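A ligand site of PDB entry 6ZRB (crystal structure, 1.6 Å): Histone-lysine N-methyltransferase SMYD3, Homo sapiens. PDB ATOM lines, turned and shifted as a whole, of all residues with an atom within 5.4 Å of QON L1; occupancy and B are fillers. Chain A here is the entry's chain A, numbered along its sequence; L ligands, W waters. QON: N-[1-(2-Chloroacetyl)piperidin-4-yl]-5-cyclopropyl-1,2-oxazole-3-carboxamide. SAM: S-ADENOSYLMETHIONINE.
The side-chain sulfur (SD) of Met 193 lies close to an oxygen (O03) of QON L1 (3.5 Å). Cys 183 touches QON L1 (O to C20, 3.4 Å). Asn 184 touches QON L1 (O to C19, 3.8 Å). O of Ser 185 touches C17 of QON L1, 3.3 Å away. CZ of Phe 186 touches C19 of QON L1, at 3.5 Å. CD1 of Ile 217 touches C06 of QON L1, at 3.8 Å. Phe 219 touches QON L1. CD1 of Ile 240 touches O15 of QON L1 (3.4 Å). Tyr 242 touches QON L1 (CD1 to O15, 3.3 Å). Tyr 260 touches QON L1. Within 4 Å of QON L1: Cys 183, Asn 184, Ser 185, Phe 186, Thr 187, Cys 189, Met 193, Ile 217, Phe 219, Ile 240, Tyr 242 and Tyr 260.
The side-chain hydroxyl of Ser 205 is in hydrogen-bond range of the side-chain amide oxygen of Asn 184 (3.2 Å). The side-chain sulfur of Cys 183 sits at hydrogen-bond distance from the side-chain amide nitrogen of Asn 184 (3.5 Å). OH of Tyr 242 is in hydrogen-bond range of O of Leu 207, at 2.6 Å.
Water W4 lies within hydrogen-bond range of O12 of QON L1, O of Ser 185 and OG1 of Thr 187. Water W1 lies within hydrogen-bond range of O of Ile 217 and O03 of QON L1. Water W2 lies within hydrogen-bond range of O03 of QON L1 (2.8 Å), N of Phe 219 (2.9 Å) and SD of Met 193 (3.7 Å). Water W3 bridges the side-chain hydroxyl of Tyr 260 and the backbone carbonyl oxygen of Ser 185.
N of Thr 187 is in hydrogen-bond range of O12 of QON L1 (2.9 Å). The side-chain sulfur of Cys 189 is bonded to a carbon (C01) of QON L1, at 1.7 Å. O of Tyr 260 lies within hydrogen-bond range of O3' of SAM L2 (2.6 Å).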
ATOM      1  N   CYS A 183      -2.393   6.705  19.494  1.00  0.00           N
ATOM      2  CA  CYS A 183      -2.974   6.564  18.141  1.00  0.00           C
ATOM      3  C   CYS A 183      -2.076   7.200  17.082  1.00  0.00           C
ATOM      4  O   CYS A 183      -2.509   7.248  15.928  1.00  0.00           O
ATOM      5  CB  CYS A 183      -4.399   7.069  18.072  1.00  0.00           C
ATOM      6  SG  CYS A 183      -4.548   8.836  18.414  1.00  0.00           S
ATOM      7  N   ASN A 184      -0.843   7.572  17.410  1.00  0.00           N
ATOM      8  CA  ASN A 184       0.094   8.174  16.420  1.00  0.00           C
ATOM      9  C   ASN A 184       1.509   7.574  16.486  1.00  0.00           C
ATOM     10  O   ASN A 184       2.319   8.001  15.678  1.00  0.00           O
ATOM     11  CB  ASN A 184       0.178   9.689  16.587  1.00  0.00           C
ATOM     12  CG  ASN A 184      -1.128  10.355  16.191  1.00  0.00           C
ATOM     13  OD1 ASN A 184      -1.408  10.472  15.000  1.00  0.00           O
ATOM     14  ND2 ASN A 184      -1.934  10.756  17.156  1.00  0.00           N
ATOM     15  N   SER A 185       1.757   6.574  17.312  1.00  0.00           N
ATOM     16  CA  SER A 185       3.056   5.856  17.395  1.00  0.00           C
ATOM     17  C   SER A 185       3.293   5.040  16.128  1.00  0.00           C
ATOM     18  O   SER A 185       2.385   4.299  15.691  1.00  0.00           O
ATOM     19  CB  SER A 185       3.105   4.942  18.587  1.00  0.00           C
ATOM     20  OG  SER A 185       3.249   5.726  19.747  1.00  0.00           O
ATOM     21  N   PHE A 186       4.509   5.108  15.599  1.00  0.00           N
ATOM     22  CA  PHE A 186       4.989   4.210  14.526  1.00  0.00           C
ATOM     23  C   PHE A 186       5.972   3.212  15.129  1.00  0.00           C
ATOM     24  O   PHE A 186       6.926   3.610  15.819  1.00  0.00           O
ATOM     25  CB  PHE A 186       5.643   4.998  13.390  1.00  0.00           C
ATOM     26  CG  PHE A 186       4.675   5.825  12.593  1.00  0.00           C
ATOM     27  CD1 PHE A 186       4.290   7.090  13.035  1.00  0.00           C
ATOM     28  CD2 PHE A 186       4.119   5.343  11.439  1.00  0.00           C
ATOM     29  CE1 PHE A 186       3.375   7.842  12.328  1.00  0.00           C
ATOM     30  CE2 PHE A 186       3.183   6.098  10.725  1.00  0.00           C
ATOM     31  CZ  PHE A 186       2.850   7.360  11.152  1.00  0.00           C
ATOM     32  N   THR A 187       5.741   1.935  14.863  1.00  0.00           N
ATOM     33  CA  THR A 187       6.682   0.855  15.185  1.00  0.00           C
ATOM     34  C   THR A 187       7.744   0.839  14.099  1.00  0.00           C
ATOM     35  O   THR A 187       7.406   0.721  12.890  1.00  0.00           O
ATOM     36  CB  THR A 187       5.970  -0.499  15.289  1.00  0.00           C
ATOM     37  OG1 THR A 187       5.004  -0.382  16.337  1.00  0.00           O
ATOM     38  CG2 THR A 187       6.946  -1.608  15.604  1.00  0.00           C
ATOM     39  N   ILE A 188       9.008   0.980  14.490  1.00  0.00           N
ATOM     40  CA  ILE A 188      10.153   1.021  13.548  1.00  0.00           C
ATOM     41  C   ILE A 188      10.659  -0.413  13.366  1.00  0.00           C
ATOM     42  O   ILE A 188      10.939  -1.108  14.370  1.00  0.00           O
ATOM     43  CB  ILE A 188      11.255   1.959  14.066  1.00  0.00           C
ATOM     44  CG1 ILE A 188      10.740   3.389  14.276  1.00  0.00           C
ATOM     45  CG2 ILE A 188      12.445   1.893  13.117  1.00  0.00           C
ATOM     46  CD1 ILE A 188      11.636   4.263  15.129  1.00  0.00           C
ATOM     47  N   CYS A 189      10.756  -0.875  12.115  1.00  0.00           N
ATOM     48  CA  CYS A 189      11.276  -2.216  11.791  1.00  0.00           C
ATOM     49  C   CYS A 189      12.688  -2.063  11.217  1.00  0.00           C
ATOM     50  O   CYS A 189      12.992  -1.051  10.542  1.00  0.00           O
ATOM     51  CB  CYS A 189      10.399  -2.939  10.794  1.00  0.00           C
ATOM     52  SG  CYS A 189       8.980  -3.584  11.663  1.00  0.00           S
ATOM     53  N   MET A 193      12.673  -6.634   8.831  1.00  0.00           N
ATOM     54  CA  MET A 193      11.232  -6.437   9.177  1.00  0.00           C
ATOM     55  C   MET A 193      10.932  -6.959  10.584  1.00  0.00           C
ATOM     56  O   MET A 193       9.785  -7.344  10.893  1.00  0.00           O
ATOM     57  CB  MET A 193      10.320  -7.076   8.116  1.00  0.00           C
ATOM     58  CG  MET A 193      10.513  -6.449   6.758  1.00  0.00           C
ATOM     59  SD  MET A 193      10.063  -4.662   6.688  1.00  0.00           S
ATOM     60  CE  MET A 193       8.367  -4.704   6.140  1.00  0.00           C
ATOM     61  N   GLN A 194      11.919  -6.856  11.471  1.00  0.00           N
ATOM     62  CA  GLN A 194      11.745  -7.095  12.915  1.00  0.00           C
ATOM     63  C   GLN A 194      11.539  -5.763  13.617  1.00  0.00           C
ATOM     64  O   GLN A 194      12.243  -4.820  13.292  1.00  0.00           O
ATOM     65  CB  GLN A 194      12.960  -7.839  13.432  1.00  0.00           C
ATOM     66  CG  GLN A 194      12.990  -9.236  12.841  1.00  0.00           C
ATOM     67  CD  GLN A 194      14.376  -9.771  12.632  1.00  0.00           C
ATOM     68  OE1 GLN A 194      15.376  -9.069  12.839  1.00  0.00           O
ATOM     69  NE2 GLN A 194      14.434 -11.030  12.205  1.00  0.00           N
ATOM     70  N   GLU A 195      10.603  -5.719  14.562  1.00  0.00           N
ATOM     71  CA  GLU A 195      10.315  -4.510  15.354  1.00  0.00           C
ATOM     72  C   GLU A 195      11.504  -4.210  16.264  1.00  0.00           C
ATOM     73  O   GLU A 195      11.911  -5.103  17.039  1.00  0.00           O
ATOM     74  CB  GLU A 195       9.039  -4.746  16.155  1.00  0.00           C
ATOM     75  CG  GLU A 195       7.849  -4.939  15.259  1.00  0.00           C
ATOM     76  CD  GLU A 195       6.499  -5.010  15.966  1.00  0.00           C
ATOM     77  OE1 GLU A 195       6.486  -4.907  17.222  1.00  0.00           O
ATOM     78  OE2 GLU A 195       5.492  -5.193  15.256  1.00  0.00           O
ATOM     79  N   SER A 205       1.717  11.153  10.361  1.00  0.00           N
ATOM     80  CA  SER A 205       0.500  10.913  11.172  1.00  0.00           C
ATOM     81  C   SER A 205      -0.746  11.445  10.490  1.00  0.00           C
ATOM     82  O   SER A 205      -1.822  11.084  10.962  1.00  0.00           O
ATOM     83  CB  SER A 205       0.589  11.533  12.535  1.00  0.00           C
ATOM     84  OG  SER A 205       1.381  10.741  13.365  1.00  0.00           O
ATOM     85  N   LEU A 207      -1.743  10.440   7.657  1.00  0.00           N
ATOM     86  CA  LEU A 207      -2.301   9.335   6.828  1.00  0.00           C
ATOM     87  C   LEU A 207      -3.380   8.582   7.605  1.00  0.00           C
ATOM     88  O   LEU A 207      -3.099   8.021   8.649  1.00  0.00           O
ATOM     89  CB  LEU A 207      -1.198   8.374   6.432  1.00  0.00           C
ATOM     90  CG  LEU A 207      -0.194   8.932   5.432  1.00  0.00           C
ATOM     91  CD1 LEU A 207       1.126   8.194   5.556  1.00  0.00           C
ATOM     92  CD2 LEU A 207      -0.761   8.849   4.020  1.00  0.00           C
ATOM     93  N   ILE A 217       4.616   2.586   4.082  1.00  0.00           N
ATOM     94  CA  ILE A 217       5.837   3.126   4.741  1.00  0.00           C
ATOM     95  C   ILE A 217       6.846   1.995   4.958  1.00  0.00           C
ATOM     96  O   ILE A 217       6.467   0.835   5.180  1.00  0.00           O
ATOM     97  CB  ILE A 217       5.476   3.851   6.045  1.00  0.00           C
ATOM     98  CG1 ILE A 217       4.817   2.926   7.054  1.00  0.00           C
ATOM     99  CG2 ILE A 217       4.637   5.073   5.736  1.00  0.00           C
ATOM    100  CD1 ILE A 217       4.703   3.526   8.443  1.00  0.00           C
ATOM    101  N   PHE A 219      10.986   1.634   6.865  1.00  0.00           N
ATOM    102  CA  PHE A 219      12.043   2.237   7.712  1.00  0.00           C
ATOM    103  C   PHE A 219      13.408   1.806   7.196  1.00  0.00           C
ATOM    104  O   PHE A 219      13.596   0.653   6.862  1.00  0.00           O
ATOM    105  CB  PHE A 219      11.847   1.827   9.163  1.00  0.00           C
ATOM    106  CG  PHE A 219      10.606   2.451   9.749  1.00  0.00           C
ATOM    107  CD1 PHE A 219      10.641   3.744  10.248  1.00  0.00           C
ATOM    108  CD2 PHE A 219       9.386   1.796   9.689  1.00  0.00           C
ATOM    109  CE1 PHE A 219       9.497   4.335  10.755  1.00  0.00           C
ATOM    110  CE2 PHE A 219       8.239   2.400  10.197  1.00  0.00           C
ATOM    111  CZ  PHE A 219       8.303   3.654  10.730  1.00  0.00           C
ATOM    112  N   ILE A 240      -2.474   4.302   4.394  1.00  0.00           N
ATOM    113  CA  ILE A 240      -1.572   3.176   4.738  1.00  0.00           C
ATOM    114  C   ILE A 240      -2.400   2.202   5.564  1.00  0.00           C
ATOM    115  O   ILE A 240      -3.457   2.614   6.091  1.00  0.00           O
ATOM    116  CB  ILE A 240      -0.324   3.650   5.487  1.00  0.00           C
ATOM    117  CG1 ILE A 240      -0.671   4.453   6.746  1.00  0.00           C
ATOM    118  CG2 ILE A 240       0.581   4.424   4.539  1.00  0.00           C
ATOM    119  CD1 ILE A 240       0.522   4.756   7.605  1.00  0.00           C
ATOM    120  N   CYS A 241      -1.948   0.963   5.650  1.00  0.00           N
ATOM    121  CA  CYS A 241      -2.511  -0.038   6.571  1.00  0.00           C
ATOM    122  C   CYS A 241      -1.783   0.074   7.925  1.00  0.00           C
ATOM    123  O   CYS A 241      -0.584  -0.156   7.985  1.00  0.00           O
ATOM    124  CB  CYS A 241      -2.420  -1.430   5.984  1.00  0.00           C
ATOM    125  SG  CYS A 241      -3.374  -2.579   6.991  1.00  0.00           S
ATOM    126  N   TYR A 242      -2.505   0.464   8.964  1.00  0.00           N
ATOM    127  CA  TYR A 242      -1.894   0.604  10.314  1.00  0.00           C
ATOM    128  C   TYR A 242      -1.534  -0.768  10.894  1.00  0.00           C
ATOM    129  O   TYR A 242      -0.813  -0.837  11.925  1.00  0.00           O
ATOM    130  CB  TYR A 242      -2.915   1.245  11.262  1.00  0.00           C
ATOM    131  CG  TYR A 242      -3.266   2.696  11.020  1.00  0.00           C
ATOM    132  CD1 TYR A 242      -2.749   3.443   9.976  1.00  0.00           C
ATOM    133  CD2 TYR A 242      -4.187   3.315  11.851  1.00  0.00           C
ATOM    134  CE1 TYR A 242      -3.107   4.773   9.793  1.00  0.00           C
ATOM    135  CE2 TYR A 242      -4.556   4.634  11.683  1.00  0.00           C
ATOM    136  CZ  TYR A 242      -3.997   5.374  10.653  1.00  0.00           C
ATOM    137  OH  TYR A 242      -4.367   6.692  10.503  1.00  0.00           O
ATOM    138  N   LEU A 243      -2.033  -1.835  10.287  1.00  0.00           N
ATOM    139  CA  LEU A 243      -2.087  -3.163  10.933  1.00  0.00           C
ATOM    140  C   LEU A 243      -1.282  -4.199  10.153  1.00  0.00           C
ATOM    141  O   LEU A 243      -1.169  -4.117   8.919  1.00  0.00           O
ATOM    142  CB  LEU A 243      -3.537  -3.627  10.991  1.00  0.00           C
ATOM    143  CG  LEU A 243      -4.481  -2.734  11.774  1.00  0.00           C
ATOM    144  CD1 LEU A 243      -5.865  -3.361  11.764  1.00  0.00           C
ATOM    145  CD2 LEU A 243      -3.976  -2.527  13.192  1.00  0.00           C
ATOM    146  N   TYR A 260      -7.345   2.943  18.034  1.00  0.00           N
ATOM    147  CA  TYR A 260      -7.546   4.070  17.083  1.00  0.00           C
ATOM    148  C   TYR A 260      -8.946   4.662  17.174  1.00  0.00           C
ATOM    149  O   TYR A 260      -9.196   5.651  16.493  1.00  0.00           O
ATOM    150  CB  TYR A 260      -7.191   3.642  15.659  1.00  0.00           C
ATOM    151  CG  TYR A 260      -5.724   3.305  15.523  1.00  0.00           C
ATOM    152  CD1 TYR A 260      -4.790   4.319  15.537  1.00  0.00           C
ATOM    153  CD2 TYR A 260      -5.269   1.993  15.430  1.00  0.00           C
ATOM    154  CE1 TYR A 260      -3.439   4.038  15.423  1.00  0.00           C
ATOM    155  CE2 TYR A 260      -3.915   1.702  15.343  1.00  0.00           C
ATOM    156  CZ  TYR A 260      -2.997   2.730  15.329  1.00  0.00           C
ATOM    157  OH  TYR A 260      -1.654   2.451  15.254  1.00  0.00           O
ATOM    158  N   VAL A 371       6.682  -6.267   3.346  1.00  0.00           N
ATOM    159  CA  VAL A 371       6.859  -7.522   4.111  1.00  0.00           C
ATOM    160  C   VAL A 371       7.082  -8.657   3.118  1.00  0.00           C
ATOM    161  O   VAL A 371       7.965  -9.498   3.375  1.00  0.00           O
ATOM    162  CB  VAL A 371       5.704  -7.784   5.086  1.00  0.00           C
ATOM    163  CG1 VAL A 371       5.714  -9.220   5.594  1.00  0.00           C
ATOM    164  CG2 VAL A 371       5.752  -6.779   6.230  1.00  0.00           C
HETATM  165  C11 QON L   1       2.962   1.287  12.131  1.00  0.00           C
HETATM  166  C13 QON L   1       1.899   2.275  11.847  1.00  0.00           C
HETATM  167  C17 QON L   1       1.407   3.311  12.675  1.00  0.00           C
HETATM  168  C19 QON L   1       0.186   6.247  13.107  1.00  0.00           C
HETATM  169  C01 QON L   1       7.818  -4.089  10.470  1.00  0.00           C
HETATM  170  C02 QON L   1       7.470  -2.848   9.740  1.00  0.00           C
HETATM  171  O03 QON L   1       8.018  -2.642   8.671  1.00  0.00           O
HETATM  172  N04 QON L   1       6.648  -1.947  10.328  1.00  0.00           N
HETATM  173  C05 QON L   1       6.585  -0.633   9.668  1.00  0.00           C
HETATM  174  C06 QON L   1       5.190  -0.077   9.664  1.00  0.00           C
HETATM  175  C07 QON L   1       4.667  -0.094  11.081  1.00  0.00           C
HETATM  176  C08 QON L   1       4.575  -1.501  11.614  1.00  0.00           C
HETATM  177  C09 QON L   1       5.956  -2.182  11.607  1.00  0.00           C
HETATM  178  N10 QON L   1       3.362   0.529  11.100  1.00  0.00           N
HETATM  179  O12 QON L   1       3.466   1.264  13.228  1.00  0.00           O
HETATM  180  N14 QON L   1       1.295   2.343  10.643  1.00  0.00           N
HETATM  181  O15 QON L   1       0.420   3.350  10.726  1.00  0.00           O
HETATM  182  C16 QON L   1       0.495   3.980  11.915  1.00  0.00           C
HETATM  183  C18 QON L   1      -0.384   5.144  12.214  1.00  0.00           C
HETATM  184  C20 QON L   1      -0.895   5.334  13.597  1.00  0.00           C
HETATM  185  N   SAM L   2      -7.350  11.630  10.913  1.00  0.00           N
HETATM  186  CA  SAM L   2      -6.137  11.839  11.748  1.00  0.00           C
HETATM  187  C   SAM L   2      -6.019  13.322  12.146  1.00  0.00           C
HETATM  188  O   SAM L   2      -4.974  13.689  12.717  1.00  0.00           O
HETATM  189  OXT SAM L   2      -7.030  14.038  11.970  1.00  0.00           O
HETATM  190  CB  SAM L   2      -4.897  11.371  10.995  1.00  0.00           C
HETATM  191  CG  SAM L   2      -4.638   9.865  11.152  1.00  0.00           C
HETATM  192  SD  SAM L   2      -4.154   9.519  12.877  1.00  0.00           S
HETATM  193  CE  SAM L   2      -2.628   8.609  12.639  1.00  0.00           C
HETATM  194  C5' SAM L   2      -5.243   8.145  13.328  1.00  0.00           C
HETATM  195  C4' SAM L   2      -6.676   8.529  13.603  1.00  0.00           C
HETATM  196  O4' SAM L   2      -7.311   8.940  12.380  1.00  0.00           O
HETATM  197  C3' SAM L   2      -7.556   7.400  14.140  1.00  0.00           C
HETATM  198  O3' SAM L   2      -7.342   7.262  15.540  1.00  0.00           O
HETATM  199  C2' SAM L   2      -8.930   7.937  13.752  1.00  0.00           C
HETATM  200  O2' SAM L   2      -9.338   9.019  14.566  1.00  0.00           O
HETATM  201  C1' SAM L   2      -8.640   8.449  12.344  1.00  0.00           C
HETATM  202  N9  SAM L   2      -8.744   7.442  11.284  1.00  0.00           N
HETATM  203  C8  SAM L   2      -7.705   6.856  10.620  1.00  0.00           C
HETATM  204  N7  SAM L   2      -8.083   6.064   9.648  1.00  0.00           N
HETATM  205  C5  SAM L   2      -9.476   6.110   9.712  1.00  0.00           C
HETATM  206  C6  SAM L   2     -10.475   5.446   8.962  1.00  0.00           C
HETATM  207  N6  SAM L   2     -10.223   4.629   7.946  1.00  0.00           N
HETATM  208  N1  SAM L   2     -11.768   5.740   9.273  1.00  0.00           N
HETATM  209  C2  SAM L   2     -12.019   6.602  10.264  1.00  0.00           C
HETATM  210  N3  SAM L   2     -11.161   7.250  11.044  1.00  0.00           N
HETATM  211  C4  SAM L   2      -9.892   6.969  10.698  1.00  0.00           C
HETATM  212  O   HOH W   1       7.132  -1.576   6.273  1.00  0.00           O
HETATM  213  O   HOH W   2      10.012  -1.028   7.564  1.00  0.00           O
HETATM  214  O   HOH W   3      -0.148   4.108  16.739  1.00  0.00           O
HETATM  215  O   HOH W   4       2.174   1.106  15.609  1.00  0.00           O
